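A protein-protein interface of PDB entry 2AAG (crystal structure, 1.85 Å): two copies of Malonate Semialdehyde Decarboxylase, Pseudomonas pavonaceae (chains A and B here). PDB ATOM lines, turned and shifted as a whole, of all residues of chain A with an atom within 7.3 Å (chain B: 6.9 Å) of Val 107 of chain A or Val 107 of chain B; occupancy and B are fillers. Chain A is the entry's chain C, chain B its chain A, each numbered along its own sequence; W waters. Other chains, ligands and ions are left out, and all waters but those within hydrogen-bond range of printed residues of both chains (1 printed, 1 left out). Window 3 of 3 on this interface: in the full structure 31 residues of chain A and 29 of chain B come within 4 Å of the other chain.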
ATOM      1  N   LEU A   2      16.964 -30.222  -6.083  1.00  0.00           N
ATOM      2  CA  LEU A   2      17.215 -30.986  -4.862  1.00  0.00           C
ATOM      3  C   LEU A   2      16.520 -30.181  -3.774  1.00  0.00           C
ATOM      4  O   LEU A   2      16.816 -28.970  -3.615  1.00  0.00           O
ATOM      5  CB  LEU A   2      18.700 -30.951  -4.571  1.00  0.00           C
ATOM      6  CG  LEU A   2      19.489 -31.912  -3.712  1.00  0.00           C
ATOM      7  CD1 LEU A   2      20.220 -31.408  -2.708  1.00  0.00           C
ATOM      8  CD2 LEU A   2      18.793 -33.040  -3.085  1.00  0.00           C
ATOM      9  N   THR A  69      15.268 -25.897   1.678  1.00  0.00           N
ATOM     10  CA  THR A  69      16.313 -25.285   0.856  1.00  0.00           C
ATOM     11  C   THR A  69      16.296 -26.022  -0.481  1.00  0.00           C
ATOM     12  O   THR A  69      16.294 -27.278  -0.500  1.00  0.00           O
ATOM     13  CB  THR A  69      17.688 -25.475   1.513  1.00  0.00           C
ATOM     14  OG1 THR A  69      17.721 -24.695   2.714  1.00  0.00           O
ATOM     15  CG2 THR A  69      18.795 -24.866   0.613  1.00  0.00           C
ATOM     16  N   VAL A  70      16.256 -25.260  -1.557  1.00  0.00           N
ATOM     17  CA  VAL A  70      16.156 -25.818  -2.891  1.00  0.00           C
ATOM     18  C   VAL A  70      17.433 -25.479  -3.651  1.00  0.00           C
ATOM     19  O   VAL A  70      17.855 -24.309  -3.633  1.00  0.00           O
ATOM     20  CB  VAL A  70      14.941 -25.227  -3.639  1.00  0.00           C
ATOM     21  CG1 VAL A  70      14.782 -25.962  -4.963  1.00  0.00           C
ATOM     22  CG2 VAL A  70      13.632 -25.377  -2.858  1.00  0.00           C
ATOM     23  N   ILE A  71      18.059 -26.477  -4.287  1.00  0.00           N
ATOM     24  CA  ILE A  71      19.060 -26.208  -5.292  1.00  0.00           C
ATOM     25  C   ILE A  71      18.463 -26.511  -6.642  1.00  0.00           C
ATOM     26  O   ILE A  71      17.986 -27.639  -6.889  1.00  0.00           O
ATOM     27  CB  ILE A  71      20.377 -27.040  -5.058  1.00  0.00           C
ATOM     28  CG1 ILE A  71      20.915 -26.800  -3.623  1.00  0.00           C
ATOM     29  CG2 ILE A  71      21.405 -26.638  -6.081  1.00  0.00           C
ATOM     30  CD1 ILE A  71      22.205 -27.705  -3.223  1.00  0.00           C
ATOM     31  N   SER A  72      18.572 -25.551  -7.537  1.00  0.00           N
ATOM     32  CA  SER A  72      17.971 -25.636  -8.855  1.00  0.00           C
ATOM     33  C   SER A  72      18.752 -24.900  -9.946  1.00  0.00           C
ATOM     34  O   SER A  72      19.346 -23.868  -9.700  1.00  0.00           O
ATOM     35  CB  SER A  72      16.566 -25.003  -8.834  1.00  0.00           C
ATOM     36  OG  SER A  72      15.983 -25.128 -10.112  1.00  0.00           O
ATOM     37  N   ARG A  73      18.683 -25.427 -11.159  1.00  0.00           N
ATOM     38  CA  ARG A  73      19.006 -24.595 -12.333  1.00  0.00           C
ATOM     39  C   ARG A  73      18.160 -23.311 -12.367  1.00  0.00           C
ATOM     40  O   ARG A  73      17.182 -23.184 -11.622  1.00  0.00           O
ATOM     41  CB  ARG A  73      18.792 -25.409 -13.601  1.00  0.00           C
ATOM     42  CG  ARG A  73      19.908 -26.443 -13.702  1.00  0.00           C
ATOM     43  CD  ARG A  73      19.889 -27.173 -15.070  1.00  0.00           C
ATOM     44  NE  ARG A  73      18.548 -27.691 -15.338  1.00  0.00           N
ATOM     45  CZ  ARG A  73      18.022 -27.892 -16.571  1.00  0.00           C
ATOM     46  NH1 ARG A  73      18.716 -27.598 -17.687  1.00  0.00           N
ATOM     47  NH2 ARG A  73      16.799 -28.419 -16.679  1.00  0.00           N
ATOM     48  N   PRO A  74      18.515 -22.325 -13.175  1.00  0.00           N
ATOM     49  CA  PRO A  74      17.734 -21.071 -13.140  1.00  0.00           C
ATOM     50  C   PRO A  74      16.246 -21.232 -13.464  1.00  0.00           C
ATOM     51  O   PRO A  74      15.869 -22.047 -14.320  1.00  0.00           O
ATOM     52  CB  PRO A  74      18.431 -20.165 -14.161  1.00  0.00           C
ATOM     53  CG  PRO A  74      19.912 -20.733 -14.173  1.00  0.00           C
ATOM     54  CD  PRO A  74      19.696 -22.224 -14.055  1.00  0.00           C
ATOM     55  N   ALA A 105      14.349 -21.161   1.006  1.00  0.00           N
ATOM     56  CA  ALA A 105      15.465 -20.457   0.417  1.00  0.00           C
ATOM     57  C   ALA A 105      15.937 -21.241  -0.830  1.00  0.00           C
ATOM     58  O   ALA A 105      16.025 -22.470  -0.752  1.00  0.00           O
ATOM     59  CB  ALA A 105      16.568 -20.359   1.389  1.00  0.00           C
ATOM     60  N   LEU A 106      16.143 -20.550  -1.954  1.00  0.00           N
ATOM     61  CA  LEU A 106      16.625 -21.198  -3.188  1.00  0.00           C
ATOM     62  C   LEU A 106      18.019 -20.753  -3.512  1.00  0.00           C
ATOM     63  O   LEU A 106      18.343 -19.588  -3.431  1.00  0.00           O
ATOM     64  CB  LEU A 106      15.783 -20.799  -4.400  1.00  0.00           C
ATOM     65  CG  LEU A 106      14.264 -20.751  -4.354  1.00  0.00           C
ATOM     66  CD1 LEU A 106      13.768 -20.481  -5.762  1.00  0.00           C
ATOM     67  CD2 LEU A 106      13.652 -22.059  -3.853  1.00  0.00           C
ATOM     68  N   VAL A 107      18.799 -21.673  -4.034  1.00  0.00           N
ATOM     69  CA  VAL A 107      20.118 -21.393  -4.533  1.00  0.00           C
ATOM     70  C   VAL A 107      20.196 -21.970  -5.974  1.00  0.00           C
ATOM     71  O   VAL A 107      19.736 -23.070  -6.245  1.00  0.00           O
ATOM     72  CB  VAL A 107      21.168 -22.045  -3.616  1.00  0.00           C
ATOM     73  CG1 VAL A 107      22.520 -21.926  -4.184  1.00  0.00           C
ATOM     74  CG2 VAL A 107      21.207 -21.325  -2.262  1.00  0.00           C
ATOM     75  N   GLU A 108      20.785 -21.181  -6.873  1.00  0.00           N
ATOM     76  CA  GLU A 108      20.850 -21.589  -8.278  1.00  0.00           C
ATOM     77  C   GLU A 108      22.217 -22.128  -8.682  1.00  0.00           C
ATOM     78  O   GLU A 108      23.257 -21.668  -8.233  1.00  0.00           O
ATOM     79  CB  GLU A 108      20.411 -20.433  -9.208  1.00  0.00           C
ATOM     80  CG  GLU A 108      18.931 -20.146  -9.018  1.00  0.00           C
ATOM     81  CD  GLU A 108      18.390 -18.991  -9.875  1.00  0.00           C
ATOM     82  OE1 GLU A 108      19.149 -18.019 -10.010  1.00  0.00           O
ATOM     83  OE2 GLU A 108      17.204 -19.035 -10.332  1.00  0.00           O
ATOM     84  N   ASN A 109      22.199 -23.057  -9.622  1.00  0.00           N
ATOM     85  CA  ASN A 109      23.431 -23.527 -10.264  1.00  0.00           C
ATOM     86  C   ASN A 109      23.163 -23.683 -11.793  1.00  0.00           C
ATOM     87  O   ASN A 109      22.189 -23.121 -12.290  1.00  0.00           O
ATOM     88  CB  ASN A 109      23.982 -24.767  -9.548  1.00  0.00           C
ATOM     89  CG  ASN A 109      23.070 -25.991  -9.684  1.00  0.00           C
ATOM     90  OD1 ASN A 109      21.991 -25.939 -10.330  1.00  0.00           O
ATOM     91  ND2 ASN A 109      23.486 -27.103  -9.038  1.00  0.00           N
ATOM     92  N   TRP A 114      25.371 -30.784 -12.323  1.00  0.00           N
ATOM     93  CA  TRP A 114      24.581 -31.919 -11.898  1.00  0.00           C
ATOM     94  C   TRP A 114      25.105 -33.199 -12.510  1.00  0.00           C
ATOM     95  O   TRP A 114      25.433 -33.241 -13.742  1.00  0.00           O
ATOM     96  CB  TRP A 114      23.117 -31.779 -12.371  1.00  0.00           C
ATOM     97  CG  TRP A 114      22.430 -30.595 -11.756  1.00  0.00           C
ATOM     98  CD1 TRP A 114      22.416 -29.280 -12.215  1.00  0.00           C
ATOM     99  CD2 TRP A 114      21.677 -30.596 -10.534  1.00  0.00           C
ATOM    100  NE1 TRP A 114      21.698 -28.490 -11.334  1.00  0.00           N
ATOM    101  CE2 TRP A 114      21.240 -29.269 -10.299  1.00  0.00           C
ATOM    102  CE3 TRP A 114      21.321 -31.617  -9.607  1.00  0.00           C
ATOM    103  CZ2 TRP A 114      20.465 -28.905  -9.159  1.00  0.00           C
ATOM    104  CZ3 TRP A 114      20.533 -31.251  -8.453  1.00  0.00           C
ATOM    105  CH2 TRP A 114      20.116 -29.912  -8.264  1.00  0.00           C
ATOM    106  N   THR B  69      27.762 -22.772   7.205  1.00  0.00           N
ATOM    107  CA  THR B  69      27.419 -22.423   5.879  1.00  0.00           C
ATOM    108  C   THR B  69      26.345 -21.325   5.940  1.00  0.00           C
ATOM    109  O   THR B  69      25.302 -21.459   6.629  1.00  0.00           O
ATOM    110  CB  THR B  69      26.855 -23.720   5.146  1.00  0.00           C
ATOM    111  OG1 THR B  69      27.920 -24.662   4.955  1.00  0.00           O
ATOM    112  CG2 THR B  69      26.476 -23.367   3.662  1.00  0.00           C
ATOM    113  N   VAL B  70      26.520 -20.287   5.115  1.00  0.00           N
ATOM    114  CA  VAL B  70      25.571 -19.142   5.158  1.00  0.00           C
ATOM    115  C   VAL B  70      24.971 -18.974   3.756  1.00  0.00           C
ATOM    116  O   VAL B  70      25.716 -18.993   2.732  1.00  0.00           O
ATOM    117  CB  VAL B  70      26.286 -17.806   5.538  1.00  0.00           C
ATOM    118  CG1 VAL B  70      25.290 -16.599   5.566  1.00  0.00           C
ATOM    119  CG2 VAL B  70      27.047 -17.909   6.892  1.00  0.00           C
ATOM    120  N   ILE B  71      23.637 -18.921   3.677  1.00  0.00           N
ATOM    121  CA  ILE B  71      22.999 -18.522   2.418  1.00  0.00           C
ATOM    122  C   ILE B  71      22.465 -17.084   2.579  1.00  0.00           C
ATOM    123  O   ILE B  71      21.725 -16.838   3.530  1.00  0.00           O
ATOM    124  CB  ILE B  71      21.805 -19.467   2.016  1.00  0.00           C
ATOM    125  CG1 ILE B  71      22.312 -20.930   1.907  1.00  0.00           C
ATOM    126  CG2 ILE B  71      21.127 -18.873   0.697  1.00  0.00           C
ATOM    127  CD1 ILE B  71      21.163 -22.013   1.591  1.00  0.00           C
ATOM    128  N   SER B  72      22.884 -16.164   1.690  1.00  0.00           N
ATOM    129  CA  SER B  72      22.542 -14.732   1.857  1.00  0.00           C
ATOM    130  C   SER B  72      22.338 -14.054   0.488  1.00  0.00           C
ATOM    131  O   SER B  72      22.930 -14.467  -0.527  1.00  0.00           O
ATOM    132  CB  SER B  72      23.704 -14.017   2.560  1.00  0.00           C
ATOM    133  OG  SER B  72      23.435 -12.647   2.734  1.00  0.00           O
ATOM    134  N   ARG B  73      21.482 -13.047   0.459  1.00  0.00           N
ATOM    135  CA  ARG B  73      21.507 -12.065  -0.640  1.00  0.00           C
ATOM    136  C   ARG B  73      22.933 -11.420  -0.708  1.00  0.00           C
ATOM    137  O   ARG B  73      23.718 -11.553   0.243  1.00  0.00           O
ATOM    138  CB  ARG B  73      20.436 -10.993  -0.385  1.00  0.00           C
ATOM    139  CG  ARG B  73      19.055 -11.526  -0.630  1.00  0.00           C
ATOM    140  CD  ARG B  73      17.993 -10.465  -0.699  1.00  0.00           C
ATOM    141  NE  ARG B  73      18.054  -9.678   0.527  1.00  0.00           N
ATOM    142  CZ  ARG B  73      17.603  -8.406   0.639  1.00  0.00           C
ATOM    143  NH1 ARG B  73      17.032  -7.757  -0.389  1.00  0.00           N
ATOM    144  NH2 ARG B  73      17.683  -7.798   1.800  1.00  0.00           N
ATOM    145  N   ALA B 105      31.666 -20.944   5.037  1.00  0.00           N
ATOM    146  CA  ALA B 105      31.425 -20.833   3.596  1.00  0.00           C
ATOM    147  C   ALA B 105      30.120 -20.084   3.373  1.00  0.00           C
ATOM    148  O   ALA B 105      29.129 -20.416   4.005  1.00  0.00           O
ATOM    149  CB  ALA B 105      31.328 -22.234   2.958  1.00  0.00           C
ATOM    150  N   LEU B 106      30.148 -19.114   2.454  1.00  0.00           N
ATOM    151  CA  LEU B 106      28.974 -18.325   2.115  1.00  0.00           C
ATOM    152  C   LEU B 106      28.540 -18.673   0.689  1.00  0.00           C
ATOM    153  O   LEU B 106      29.387 -18.849  -0.227  1.00  0.00           O
ATOM    154  CB  LEU B 106      29.294 -16.829   2.113  1.00  0.00           C
ATOM    155  CG  LEU B 106      30.004 -16.187   3.330  1.00  0.00           C
ATOM    156  CD1 LEU B 106      29.942 -14.689   3.115  1.00  0.00           C
ATOM    157  CD2 LEU B 106      29.353 -16.455   4.670  1.00  0.00           C
ATOM    158  N   VAL B 107      27.214 -18.672   0.487  1.00  0.00           N
ATOM    159  CA  VAL B 107      26.672 -18.839  -0.837  1.00  0.00           C
ATOM    160  C   VAL B 107      25.629 -17.741  -1.057  1.00  0.00           C
ATOM    161  O   VAL B 107      24.832 -17.398  -0.129  1.00  0.00           O
ATOM    162  CB  VAL B 107      26.021 -20.247  -0.949  1.00  0.00           C
ATOM    163  CG1 VAL B 107      25.286 -20.382  -2.246  1.00  0.00           C
ATOM    164  CG2 VAL B 107      27.157 -21.318  -0.921  1.00  0.00           C
ATOM    165  N   GLU B 108      25.595 -17.203  -2.276  1.00  0.00           N
ATOM    166  CA  GLU B 108      24.723 -16.059  -2.579  1.00  0.00           C
ATOM    167  C   GLU B 108      23.465 -16.431  -3.383  1.00  0.00           C
ATOM    168  O   GLU B 108      23.529 -17.186  -4.338  1.00  0.00           O
ATOM    169  CB  GLU B 108      25.500 -14.925  -3.242  1.00  0.00           C
ATOM    170  CG  GLU B 108      26.418 -14.224  -2.161  1.00  0.00           C
ATOM    171  CD  GLU B 108      27.315 -13.095  -2.694  1.00  0.00           C
ATOM    172  OE1 GLU B 108      27.745 -13.217  -3.885  1.00  0.00           O
ATOM    173  OE2 GLU B 108      27.591 -12.089  -1.941  1.00  0.00           O
ATOM    174  N   ASN B 109      22.362 -15.813  -3.016  1.00  0.00           N
ATOM    175  CA  ASN B 109      21.192 -15.882  -3.878  1.00  0.00           C
ATOM    176  C   ASN B 109      20.652 -14.461  -4.088  1.00  0.00           C
ATOM    177  O   ASN B 109      21.394 -13.492  -3.882  1.00  0.00           O
ATOM    178  CB  ASN B 109      20.168 -16.908  -3.373  1.00  0.00           C
ATOM    179  CG  ASN B 109      19.628 -16.567  -2.017  1.00  0.00           C
ATOM    180  OD1 ASN B 109      19.936 -15.485  -1.476  1.00  0.00           O
ATOM    181  ND2 ASN B 109      18.732 -17.442  -1.484  1.00  0.00           N
ATOM    182  N   ASP B 113      14.608 -15.342  -4.272  1.00  0.00           N
ATOM    183  CA  ASP B 113      14.988 -16.670  -3.787  1.00  0.00           C
ATOM    184  C   ASP B 113      14.638 -16.955  -2.380  1.00  0.00           C
ATOM    185  O   ASP B 113      15.184 -17.918  -1.823  1.00  0.00           O
ATOM    186  CB  ASP B 113      16.500 -16.888  -4.022  1.00  0.00           C
ATOM    187  CG  ASP B 113      16.839 -16.811  -5.476  1.00  0.00           C
ATOM    188  OD1 ASP B 113      16.026 -17.368  -6.251  1.00  0.00           O
ATOM    189  OD2 ASP B 113      17.889 -16.302  -5.959  1.00  0.00           O
ATOM    190  N   TRP B 114      13.701 -16.152  -1.812  1.00  0.00           N
ATOM    191  CA  TRP B 114      13.314 -16.272  -0.425  1.00  0.00           C
ATOM    192  C   TRP B 114      11.833 -16.194  -0.261  1.00  0.00           C
ATOM    193  O   TRP B 114      11.192 -15.343  -0.886  1.00  0.00           O
ATOM    194  CB  TRP B 114      13.927 -15.167   0.491  1.00  0.00           C
ATOM    195  CG  TRP B 114      15.412 -15.142   0.499  1.00  0.00           C
ATOM    196  CD1 TRP B 114      16.248 -14.514  -0.367  1.00  0.00           C
ATOM    197  CD2 TRP B 114      16.220 -15.867   1.388  1.00  0.00           C
ATOM    198  NE1 TRP B 114      17.556 -14.779  -0.027  1.00  0.00           N
ATOM    199  CE2 TRP B 114      17.571 -15.596   1.067  1.00  0.00           C
ATOM    200  CE3 TRP B 114      15.942 -16.694   2.473  1.00  0.00           C
ATOM    201  CZ2 TRP B 114      18.671 -16.171   1.778  1.00  0.00           C
ATOM    202  CZ3 TRP B 114      17.042 -17.255   3.218  1.00  0.00           C
ATOM    203  CH2 TRP B 114      18.377 -16.990   2.831  1.00  0.00           C
HETATM  204  O   HOH W   1      19.874 -17.028  -7.381  1.00  0.00           O
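N of Leu 106 of chain A lies within hydrogen-bond range of O of Asp 113 of chain B (2.8 Å).
The side-chain amide nitrogen of Asn 109 of chain B lies within hydrogen-bond range of the backbone carbonyl oxygen of Leu 106 of chain A (2.9 Å).
N of Val 70 of chain A sits at hydrogen-bond distance from O of Ala 105 of chain A (2.9 Å).
O of Val 70 of chain B lies within hydrogen-bond range of N of Val 107 of chain B (2.7 Å).
The backbone carbonyl oxygen (O) of Ser 72 of chain B lies within hydrogen-bond range of the backbone NH (N) of Asn 109 of chain B, 2.9 Å away.
The backbone NH (N) of Arg 73 of chain B sits at hydrogen-bond distance from the side-chain amide oxygen (OD1) of Asn 109 of chain B, 3.5 Å away.
The backbone NH of Ser 72 of chain A lies within hydrogen-bond range of the backbone carbonyl oxygen of Val 107 of chain A, 3.0 Å away.
The backbone carbonyl oxygen (O) of Val 70 of chain A sits at hydrogen-bond distance from the backbone NH (N) of Val 107 of chain A (2.8 Å).
Thr 69 of chain A touches Ile 71 of chain B.
O of Asp 113 of chain B touches CA of Ala 105 of chain A (3.4 Å).
CZ3 of Trp 114 of chain B touches CB of Ala 105 of chain A, 3.6 Å away.
CG2 of Val 107 of chain A touches CG2 of Ile 71 of chain B (3.8 Å).
Val 107 of chain A touches Val 107 of chain B (CG1 to CG1, 3.7 Å).
Of the printed residues of chain B, Thr 69 of chain A touches Ile 71 (3.8 Å).
Val 70 of chain A touches none of the printed residues of chain B.
Val 107 of chain A touches just these residues of chain B: Ile 71 and Val 107.
Trp 114 of chain A touches none of the printed residues of chain B.
Val 107 of chain B touches one residue of chain A.
Printed residues of chain A within 4 Å of Asn 109 of chain B: Leu 106 (2.9 Å).
Of the printed residues of chain A, Asp 113 of chain B touches Ala 105 (3.4 Å) and Leu 106 (2.8 Å).
Of the printed residues of chain A, Trp 114 of chain B touches Ala 105.
The nearest residue of chain B that does not touch Val 107 of chain A is Asn 109 of chain B (4.6 Å).
The nearest printed residue of chain A that does not touch Ile 71 of chain B is Ala 105 of chain A (4.8 Å).
Of the 12 printed residues of chain B, 5 touch a printed residue of chain A.
Printed residues of chain B that touch a printed residue of chain A: Ile 71, Val 107, Asn 109, Asp 113 and Trp 114.
Printed residues of chain A that touch a printed residue of chain B: Thr 69, Ala 105, Leu 106 and Val 107.
Hydrophobic or aromatic side chains of chain A within 4 Å of the printed part of chain B: Ala 105, Leu 106 and Val 107.
Among the printed residues, 7 pairs touch across the chains.
Thr 69 of chain A touches Ile 71 of chain B, but with the chains exchanged Ile 71 of chain A does not touch Thr 69 of chain B (9.2 Å).
Ala 105 of chain A touches Trp 114 of chain B, but with the chains exchanged Trp 114 of chain A does not touch Ala 105 of chain B (17.6 Å).
Leu 106 of chain A touches Asn 109 of chain B, but with the chains exchanged Asn 109 of chain A does not touch Leu 106 of chain B (12.3 Å).
Val 107 of chain A touches Ile 71 of chain B, but with the chains exchanged Ile 71 of chain A does not touch Val 107 of chain B (7.9 Å).
Positions printed for both chains: 69, 70, 71, 72, 73, 105, 106, 107, 108, 109 and 114.
Water W1 lies within hydrogen-bond range of OD2 of Asp 113 of chain B (2.5 Å) and OE1 of Glu 108 of chain A (2.9 Å).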
